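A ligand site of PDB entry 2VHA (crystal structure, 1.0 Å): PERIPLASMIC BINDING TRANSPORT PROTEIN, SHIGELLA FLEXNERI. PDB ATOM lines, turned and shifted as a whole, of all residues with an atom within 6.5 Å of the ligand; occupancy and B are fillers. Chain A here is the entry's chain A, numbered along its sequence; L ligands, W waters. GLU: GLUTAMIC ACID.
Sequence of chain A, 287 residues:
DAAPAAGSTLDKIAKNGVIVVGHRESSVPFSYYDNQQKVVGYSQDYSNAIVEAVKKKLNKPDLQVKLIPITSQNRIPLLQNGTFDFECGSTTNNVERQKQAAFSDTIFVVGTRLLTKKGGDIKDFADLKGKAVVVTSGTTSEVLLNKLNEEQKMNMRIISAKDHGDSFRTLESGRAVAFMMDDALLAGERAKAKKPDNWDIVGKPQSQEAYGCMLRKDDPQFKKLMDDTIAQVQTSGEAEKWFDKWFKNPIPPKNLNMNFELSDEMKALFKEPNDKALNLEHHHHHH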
ATOM      1  N   ARG A  24      22.356 -14.017  -6.021  1.00  0.00           N
ATOM      2  CA  ARG A  24      21.124 -14.559  -5.387  1.00  0.00           C
ATOM      3  C   ARG A  24      19.963 -14.443  -6.352  1.00  0.00           C
ATOM      4  O   ARG A  24      19.934 -13.683  -7.342  1.00  0.00           O
ATOM      5  CB  ARG A  24      20.848 -13.822  -4.075  1.00  0.00           C
ATOM      6  CG  ARG A  24      22.035 -13.838  -3.126  1.00  0.00           C
ATOM      7  CD  ARG A  24      22.485 -15.252  -2.761  1.00  0.00           C
ATOM      8  NE  ARG A  24      21.395 -15.949  -2.060  1.00  0.00           N
ATOM      9  CZ  ARG A  24      21.150 -15.879  -0.773  1.00  0.00           C
ATOM     10  NH1 ARG A  24      21.944 -15.251   0.054  1.00  0.00           N
ATOM     11  NH2 ARG A  24      20.068 -16.471  -0.265  1.00  0.00           N
ATOM     12  N   SER A  27      17.086 -12.215  -2.976  1.00  0.00           N
ATOM     13  CA  SER A  27      17.525 -11.383  -1.863  1.00  0.00           C
ATOM     14  C   SER A  27      17.188  -9.954  -2.218  1.00  0.00           C
ATOM     15  O   SER A  27      18.004  -9.234  -2.845  1.00  0.00           O
ATOM     16  CB  SER A  27      19.004 -11.559  -1.579  1.00  0.00           C
ATOM     17  OG  SER A  27      19.244 -12.816  -0.987  1.00  0.00           O
ATOM     18  N   THR A  71      22.782 -20.207  -3.133  1.00  0.00           N
ATOM     19  CA  THR A  71      21.845 -20.098  -2.021  1.00  0.00           C
ATOM     20  C   THR A  71      22.553 -19.826  -0.725  1.00  0.00           C
ATOM     21  O   THR A  71      23.781 -19.955  -0.585  1.00  0.00           O
ATOM     22  CB  THR A  71      20.943 -21.335  -1.906  1.00  0.00           C
ATOM     23  OG1 THR A  71      21.924 -22.413  -1.436  1.00  0.00           O
ATOM     24  CG2 THR A  71      20.248 -21.742  -3.165  1.00  0.00           C
ATOM     25  N   SER A  72      21.755 -19.510   0.317  1.00  0.00           N
ATOM     26  CA  SER A  72      22.352 -19.303   1.633  1.00  0.00           C
ATOM     27  C   SER A  72      23.032 -20.562   2.114  1.00  0.00           C
ATOM     28  O   SER A  72      24.052 -20.558   2.787  1.00  0.00           O
ATOM     29  CB  SER A  72      21.255 -18.886   2.625  1.00  0.00           C
ATOM     30  OG  SER A  72      20.773 -17.555   2.315  1.00  0.00           O
ATOM     31  N   ARG A  75      26.390 -21.533  -0.500  1.00  0.00           N
ATOM     32  CA  ARG A  75      27.362 -20.546  -0.971  1.00  0.00           C
ATOM     33  C   ARG A  75      28.796 -20.838  -0.549  1.00  0.00           C
ATOM     34  O   ARG A  75      29.699 -20.657  -1.372  1.00  0.00           O
ATOM     35  CB  ARG A  75      26.942 -19.139  -0.526  1.00  0.00           C
ATOM     36  CG  ARG A  75      26.756 -19.001   0.975  1.00  0.00           C
ATOM     37  CD  ARG A  75      26.300 -17.622   1.457  1.00  0.00           C
ATOM     38  NE  ARG A  75      25.705 -17.763   2.784  1.00  0.00           N
ATOM     39  CZ  ARG A  75      24.728 -17.033   3.252  1.00  0.00           C
ATOM     40  NH1 ARG A  75      24.315 -15.959   2.628  1.00  0.00           N
ATOM     41  NH2 ARG A  75      24.129 -17.426   4.377  1.00  0.00           N
ATOM     42  N   GLY A  89      25.628  -9.867  -2.182  1.00  0.00           N
ATOM     43  CA  GLY A  89      24.215 -10.157  -1.988  1.00  0.00           C
ATOM     44  C   GLY A  89      23.771  -9.751  -0.628  1.00  0.00           C
ATOM     45  O   GLY A  89      23.704  -8.579  -0.238  1.00  0.00           O
ATOM     46  N   SER A  90      23.463 -10.789   0.175  1.00  0.00           N
ATOM     47  CA  SER A  90      22.919 -10.650   1.512  1.00  0.00           C
ATOM     48  C   SER A  90      23.621 -11.587   2.486  1.00  0.00           C
ATOM     49  O   SER A  90      22.989 -12.099   3.408  1.00  0.00           O
ATOM     50  CB  SER A  90      21.399 -10.810   1.524  1.00  0.00           C
ATOM     51  OG  SER A  90      21.032 -12.092   1.000  1.00  0.00           O
ATOM     52  N   THR A  91      24.920 -11.821   2.286  1.00  0.00           N
ATOM     53  CA  THR A  91      25.676 -12.672   3.199  1.00  0.00           C
ATOM     54  C   THR A  91      26.246 -11.896   4.364  1.00  0.00           C
ATOM     55  O   THR A  91      27.035 -10.952   4.180  1.00  0.00           O
ATOM     56  CB  THR A  91      26.804 -13.414   2.462  1.00  0.00           C
ATOM     57  OG1 THR A  91      26.244 -14.106   1.348  1.00  0.00           O
ATOM     58  CG2 THR A  91      27.506 -14.380   3.387  1.00  0.00           C
ATOM     59  N   THR A  92      25.913 -12.331   5.586  1.00  0.00           N
ATOM     60  CA  THR A  92      26.495 -11.788   6.807  1.00  0.00           C
ATOM     61  C   THR A  92      27.946 -12.207   6.921  1.00  0.00           C
ATOM     62  O   THR A  92      28.321 -13.369   6.822  1.00  0.00           O
ATOM     63  CB  THR A  92      25.710 -12.279   8.033  1.00  0.00           C
ATOM     64  OG1 THR A  92      24.414 -11.692   7.932  1.00  0.00           O
ATOM     65  CG2 THR A  92      26.417 -11.834   9.308  1.00  0.00           C
ATOM     66  N   ASN A  93      28.780 -11.228   7.196  1.00  0.00           N
ATOM     67  CA  ASN A  93      30.165 -11.378   7.626  1.00  0.00           C
ATOM     68  C   ASN A  93      30.174 -11.650   9.101  1.00  0.00           C
ATOM     69  O   ASN A  93      29.780 -10.771   9.881  1.00  0.00           O
ATOM     70  CB  ASN A  93      30.933 -10.085   7.287  1.00  0.00           C
ATOM     71  CG  ASN A  93      32.324 -10.022   7.843  1.00  0.00           C
ATOM     72  OD1 ASN A  93      32.789 -10.977   8.470  1.00  0.00           O
ATOM     73  ND2 ASN A  93      32.978  -8.877   7.614  1.00  0.00           N
ATOM     74  N   ARG A  97      32.238 -17.559   9.925  1.00  0.00           N
ATOM     75  CA  ARG A  97      32.420 -17.701   8.457  1.00  0.00           C
ATOM     76  C   ARG A  97      33.770 -17.263   7.964  1.00  0.00           C
ATOM     77  O   ARG A  97      34.244 -17.711   6.930  1.00  0.00           O
ATOM     78  CB  ARG A  97      31.303 -16.940   7.747  1.00  0.00           C
ATOM     79  CG  ARG A  97      29.952 -17.565   7.956  1.00  0.00           C
ATOM     80  CD  ARG A  97      28.853 -16.683   7.421  1.00  0.00           C
ATOM     81  NE  ARG A  97      27.551 -17.331   7.608  1.00  0.00           N
ATOM     82  CZ  ARG A  97      26.395 -16.834   7.202  1.00  0.00           C
ATOM     83  NH1 ARG A  97      26.395 -15.661   6.597  1.00  0.00           N
ATOM     84  NH2 ARG A  97      25.254 -17.466   7.383  1.00  0.00           N
ATOM     85  N   VAL A 110      21.742  -5.020   8.848  1.00  0.00           N
ATOM     86  CA  VAL A 110      20.366  -5.477   9.096  1.00  0.00           C
ATOM     87  C   VAL A 110      20.207  -5.923  10.529  1.00  0.00           C
ATOM     88  O   VAL A 110      21.165  -6.222  11.255  1.00  0.00           O
ATOM     89  CB  VAL A 110      19.992  -6.646   8.148  1.00  0.00           C
ATOM     90  CG1 VAL A 110      20.097  -6.219   6.685  1.00  0.00           C
ATOM     91  CG2 VAL A 110      20.846  -7.878   8.448  1.00  0.00           C
ATOM     92  N   THR A 112      17.673  -8.899  12.612  1.00  0.00           N
ATOM     93  CA  THR A 112      16.865 -10.091  12.340  1.00  0.00           C
ATOM     94  C   THR A 112      15.530 -10.003  13.090  1.00  0.00           C
ATOM     95  O   THR A 112      15.490  -9.957  14.325  1.00  0.00           O
ATOM     96  CB  THR A 112      17.675 -11.337  12.695  1.00  0.00           C
ATOM     97  OG1 THR A 112      18.214 -11.222  14.018  1.00  0.00           O
ATOM     98  CG2 THR A 112      18.776 -11.558  11.664  1.00  0.00           C
ATOM     99  N   THR A 136      14.885 -19.367   6.313  1.00  0.00           N
ATOM    100  CA  THR A 136      15.603 -19.874   5.163  1.00  0.00           C
ATOM    101  C   THR A 136      16.790 -20.700   5.640  1.00  0.00           C
ATOM    102  O   THR A 136      17.563 -20.329   6.529  1.00  0.00           O
ATOM    103  CB  THR A 136      16.074 -18.719   4.271  1.00  0.00           C
ATOM    104  OG1 THR A 136      14.930 -17.938   3.953  1.00  0.00           O
ATOM    105  CG2 THR A 136      16.844 -19.207   3.066  1.00  0.00           C
ATOM    106  N   SER A 137      16.949 -21.876   5.024  1.00  0.00           N
ATOM    107  CA  SER A 137      18.024 -22.775   5.314  1.00  0.00           C
ATOM    108  C   SER A 137      19.377 -22.056   5.149  1.00  0.00           C
ATOM    109  O   SER A 137      19.583 -21.331   4.171  1.00  0.00           O
ATOM    110  CB  SER A 137      18.017 -24.003   4.415  1.00  0.00           C
ATOM    111  OG  SER A 137      16.800 -24.737   4.520  1.00  0.00           O
ATOM    112  N   GLY A 138      20.300 -22.367   6.078  1.00  0.00           N
ATOM    113  CA  GLY A 138      21.683 -21.944   5.884  1.00  0.00           C
ATOM    114  C   GLY A 138      21.969 -20.532   6.317  1.00  0.00           C
ATOM    115  O   GLY A 138      23.038 -19.980   6.019  1.00  0.00           O
ATOM    116  N   THR A 139      21.019 -19.893   7.024  1.00  0.00           N
ATOM    117  CA  THR A 139      21.157 -18.517   7.441  1.00  0.00           C
ATOM    118  C   THR A 139      21.468 -18.375   8.922  1.00  0.00           C
ATOM    119  O   THR A 139      21.249 -19.267   9.776  1.00  0.00           O
ATOM    120  CB  THR A 139      19.852 -17.751   7.129  1.00  0.00           C
ATOM    121  OG1 THR A 139      18.773 -18.288   7.909  1.00  0.00           O
ATOM    122  CG2 THR A 139      19.549 -17.711   5.648  1.00  0.00           C
ATOM    123  N   THR A 140      21.945 -17.168   9.262  1.00  0.00           N
ATOM    124  CA  THR A 140      22.165 -16.791  10.657  1.00  0.00           C
ATOM    125  C   THR A 140      20.832 -16.845  11.414  1.00  0.00           C
ATOM    126  O   THR A 140      20.808 -17.200  12.609  1.00  0.00           O
ATOM    127  CB  THR A 140      22.863 -15.433  10.801  1.00  0.00           C
ATOM    128  OG1 THR A 140      22.143 -14.549   9.948  1.00  0.00           O
ATOM    129  CG2 THR A 140      24.287 -15.494  10.364  1.00  0.00           C
ATOM    130  N   SER A 141      19.725 -16.504  10.779  1.00  0.00           N
ATOM    131  CA  SER A 141      18.422 -16.569  11.436  1.00  0.00           C
ATOM    132  C   SER A 141      18.074 -18.001  11.798  1.00  0.00           C
ATOM    133  O   SER A 141      17.504 -18.252  12.873  1.00  0.00           O
ATOM    134  CB  SER A 141      17.308 -15.907  10.614  1.00  0.00           C
ATOM    135  OG  SER A 141      17.380 -14.482  10.665  1.00  0.00           O
ATOM    136  N   ASP A 163      14.952 -20.795   0.000  1.00  0.00           N
ATOM    137  CA  ASP A 163      15.336 -19.403  -0.308  1.00  0.00           C
ATOM    138  C   ASP A 163      14.275 -18.497   0.243  1.00  0.00           C
ATOM    139  O   ASP A 163      13.206 -18.927   0.690  1.00  0.00           O
ATOM    140  CB  ASP A 163      15.619 -19.215  -1.780  1.00  0.00           C
ATOM    141  CG  ASP A 163      16.642 -18.150  -2.129  1.00  0.00           C
ATOM    142  OD1 ASP A 163      17.030 -18.086  -3.321  1.00  0.00           O
ATOM    143  OD2 ASP A 163      17.092 -17.408  -1.193  1.00  0.00           O
ATOM    144  N   HIS A 164      14.560 -17.183   0.219  1.00  0.00           N
ATOM    145  CA  HIS A 164      13.704 -16.241   0.917  1.00  0.00           C
ATOM    146  C   HIS A 164      12.291 -16.187   0.353  1.00  0.00           C
ATOM    147  O   HIS A 164      11.331 -16.034   1.116  1.00  0.00           O
ATOM    148  CB  HIS A 164      14.361 -14.844   0.976  1.00  0.00           C
ATOM    149  CG  HIS A 164      15.737 -14.941   1.584  1.00  0.00           C
ATOM    150  ND1 HIS A 164      15.987 -15.603   2.775  1.00  0.00           N
ATOM    151  CD2 HIS A 164      16.899 -14.387   1.105  1.00  0.00           C
ATOM    152  CE1 HIS A 164      17.277 -15.471   2.981  1.00  0.00           C
ATOM    153  NE2 HIS A 164      17.867 -14.770   2.002  1.00  0.00           N
ATOM    154  N   MET A 181      13.757 -13.386   9.461  1.00  0.00           N
ATOM    155  CA  MET A 181      14.859 -13.068   8.554  1.00  0.00           C
ATOM    156  C   MET A 181      15.304 -11.640   8.809  1.00  0.00           C
ATOM    157  O   MET A 181      14.615 -10.829   9.441  1.00  0.00           O
ATOM    158  CB  MET A 181      14.491 -13.265   7.090  1.00  0.00           C
ATOM    159  CG  MET A 181      15.643 -13.341   6.090  1.00  0.00           C
ATOM    160  SD  MET A 181      17.044 -14.338   6.541  1.00  0.00           S
ATOM    161  CE  MET A 181      16.244 -15.923   6.784  1.00  0.00           C
ATOM    162  N   ASP A 182      16.488 -11.312   8.245  1.00  0.00           N
ATOM    163  CA  ASP A 182      16.970  -9.968   8.121  1.00  0.00           C
ATOM    164  C   ASP A 182      15.823  -9.045   7.709  1.00  0.00           C
ATOM    165  O   ASP A 182      15.126  -9.304   6.704  1.00  0.00           O
ATOM    166  CB  ASP A 182      18.035  -9.899   7.044  1.00  0.00           C
ATOM    167  CG  ASP A 182      19.189 -10.861   7.163  1.00  0.00           C
ATOM    168  OD1 ASP A 182      19.200 -11.696   8.097  1.00  0.00           O
ATOM    169  OD2 ASP A 182      20.121 -10.760   6.332  1.00  0.00           O
ATOM    170  N   LEU A 185      15.424  -7.958   4.013  1.00  0.00           N
ATOM    171  CA  LEU A 185      14.948  -9.068   3.156  1.00  0.00           C
ATOM    172  C   LEU A 185      13.477  -9.329   3.344  1.00  0.00           C
ATOM    173  O   LEU A 185      12.782  -9.679   2.348  1.00  0.00           O
ATOM    174  CB  LEU A 185      15.774 -10.334   3.435  1.00  0.00           C
ATOM    175  CG  LEU A 185      17.255 -10.270   3.055  1.00  0.00           C
ATOM    176  CD1 LEU A 185      17.961 -11.527   3.483  1.00  0.00           C
ATOM    177  CD2 LEU A 185      17.407 -10.081   1.539  1.00  0.00           C
ATOM    178  N   GLU A 209      23.661  -7.415  12.035  1.00  0.00           N
ATOM    179  CA  GLU A 209      24.571  -8.140  11.157  1.00  0.00           C
ATOM    180  C   GLU A 209      24.992  -7.243   9.957  1.00  0.00           C
ATOM    181  O   GLU A 209      24.195  -6.502   9.397  1.00  0.00           O
ATOM    182  CB  GLU A 209      23.918  -9.415  10.641  1.00  0.00           C
ATOM    183  CG  GLU A 209      23.522 -10.323  11.787  1.00  0.00           C
ATOM    184  CD  GLU A 209      22.979 -11.691  11.406  1.00  0.00           C
ATOM    185  OE1 GLU A 209      23.090 -12.113  10.205  1.00  0.00           O
ATOM    186  OE2 GLU A 209      22.386 -12.370  12.305  1.00  0.00           O
ATOM    187  N   ALA A 210      26.258  -7.372   9.620  1.00  0.00           N
ATOM    188  CA  ALA A 210      26.868  -6.695   8.498  1.00  0.00           C
ATOM    189  C   ALA A 210      26.920  -7.573   7.245  1.00  0.00           C
ATOM    190  O   ALA A 210      27.433  -8.681   7.331  1.00  0.00           O
ATOM    191  CB  ALA A 210      28.315  -6.247   8.840  1.00  0.00           C
ATOM    192  N   TYR A 211      26.459  -7.071   6.116  1.00  0.00           N
ATOM    193  CA  TYR A 211      26.643  -7.719   4.845  1.00  0.00           C
ATOM    194  C   TYR A 211      28.017  -7.320   4.248  1.00  0.00           C
ATOM    195  O   TYR A 211      28.332  -6.125   4.195  1.00  0.00           O
ATOM    196  CB  TYR A 211      25.605  -7.278   3.834  1.00  0.00           C
ATOM    197  CG  TYR A 211      24.195  -7.732   4.030  1.00  0.00           C
ATOM    198  CD1 TYR A 211      23.815  -8.545   5.075  1.00  0.00           C
ATOM    199  CD2 TYR A 211      23.214  -7.331   3.131  1.00  0.00           C
ATOM    200  CE1 TYR A 211      22.474  -8.949   5.228  1.00  0.00           C
ATOM    201  CE2 TYR A 211      21.888  -7.711   3.252  1.00  0.00           C
ATOM    202  CZ  TYR A 211      21.523  -8.539   4.322  1.00  0.00           C
ATOM    203  OH  TYR A 211      20.201  -8.930   4.417  1.00  0.00           O
HETATM  204  N   GLU L   1      22.343 -12.410   6.125  1.00  0.00           N
HETATM  205  CA  GLU L   1      21.880 -13.760   6.512  1.00  0.00           C
HETATM  206  C   GLU L   1      22.966 -14.788   6.291  1.00  0.00           C
HETATM  207  O   GLU L   1      24.028 -14.425   5.732  1.00  0.00           O
HETATM  208  CB  GLU L   1      20.562 -14.110   5.936  1.00  0.00           C
HETATM  209  CG  GLU L   1      20.343 -13.774   4.588  1.00  0.00           C
HETATM  210  CD  GLU L   1      21.013 -14.632   3.615  1.00  0.00           C
HETATM  211  OE1 GLU L   1      21.826 -15.535   3.859  1.00  0.00           O
HETATM  212  OE2 GLU L   1      20.663 -14.304   2.493  1.00  0.00           O
HETATM  213  OXT GLU L   1      22.796 -15.933   6.795  1.00  0.00           O
HETATM  214  O   HOH W   1      19.585 -14.148   9.099  1.00  0.00           O
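An oxygen (OE2) of the ligand lies within salt-bridge range of the guanidinium group of Arg 24 (2.9 Å).
A nitrogen (N) of the ligand sits at hydrogen-bond distance from the backbone carbonyl oxygen (O) of Ser 90 (2.8 Å).
N of Thr 140 lies within hydrogen-bond range of OXT of the ligand, 2.9 Å away.
An oxygen (OE2) of the ligand lies within hydrogen-bond range of a ring nitrogen (NE2) of His 164 (2.9 Å).
NH1 of Arg 97 is in salt-bridge range of O of the ligand (2.8 Å).
A nitrogen (N) of the ligand lies within hydrogen-bond range of the side-chain hydroxyl (OG1) of Thr 92 (2.8 Å).
A nitrogen (N) of the ligand lies within salt-bridge range of the side-chain carboxylate of Asp 182 (2.8 Å).
O of the ligand sits at hydrogen-bond distance from N of Thr 92, 2.8 Å away.
NH1 of Arg 75 is in salt-bridge range of OE1 of the ligand.
An oxygen (OE1) of the ligand sits at hydrogen-bond distance from the side-chain hydroxyl (OG) of Ser 72 (2.8 Å).
OE2 of the ligand lies within hydrogen-bond range of OG of Ser 90, 2.7 Å away.
The guanidinium group of Arg 24 is in hydrogen-bond range of the side-chain hydroxyl of Ser 72 (2.9 Å).
NE of Arg 75 is in hydrogen-bond range of O of Ser 72 (3.2 Å).
The side-chain hydroxyl (OG1) of Thr 136 sits at hydrogen-bond distance from a ring nitrogen (ND1) of His 164 (2.8 Å).
OD2 of Asp 163 is in salt-bridge range of NH2 of Arg 24 (3.3 Å).
The guanidinium group (NH1) of Arg 75 is in hydrogen-bond range of the side-chain hydroxyl (OG1) of Thr 91 (3.0 Å).
The guanidinium group (NH2) of Arg 75 lies within hydrogen-bond range of the backbone carbonyl oxygen (O) of Gly 138 (3.2 Å).
OG1 of Thr 139 lies within hydrogen-bond range of O of Thr 136, 2.7 Å away.
The side-chain hydroxyl (OG) of Ser 27 is in hydrogen-bond range of the side-chain hydroxyl (OG) of Ser 90 (2.8 Å).
Thr 91 touches the ligand.
Thr 139 touches the ligand.
Met 181 touches the ligand.
CD1 of Leu 185 touches CG of the ligand, 3.5 Å away.
Tyr 211 touches the ligand (CE1 to N, 3.6 Å).
14 residues have an atom within 4 Å of the ligand: Arg 24, Ser 72, Arg 75, Ser 90, Thr 91, Thr 92, Arg 97, Thr 139, Thr 140, His 164, Met 181, Asp 182, Leu 185 and Tyr 211.
The nearest printed residue that does not touch the ligand is Ser 27 (4.04 Å).
Water W1 lies within hydrogen-bond range of the side-chain carboxylate (OD1) of Asp 182 (2.7 Å), the side-chain hydroxyl (OG1) of Thr 140 (2.7 Å), the side-chain hydroxyl (OG) of Ser 141 (2.7 Å) and the side-chain sulfur (SD) of Met 181 (3.6 Å).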
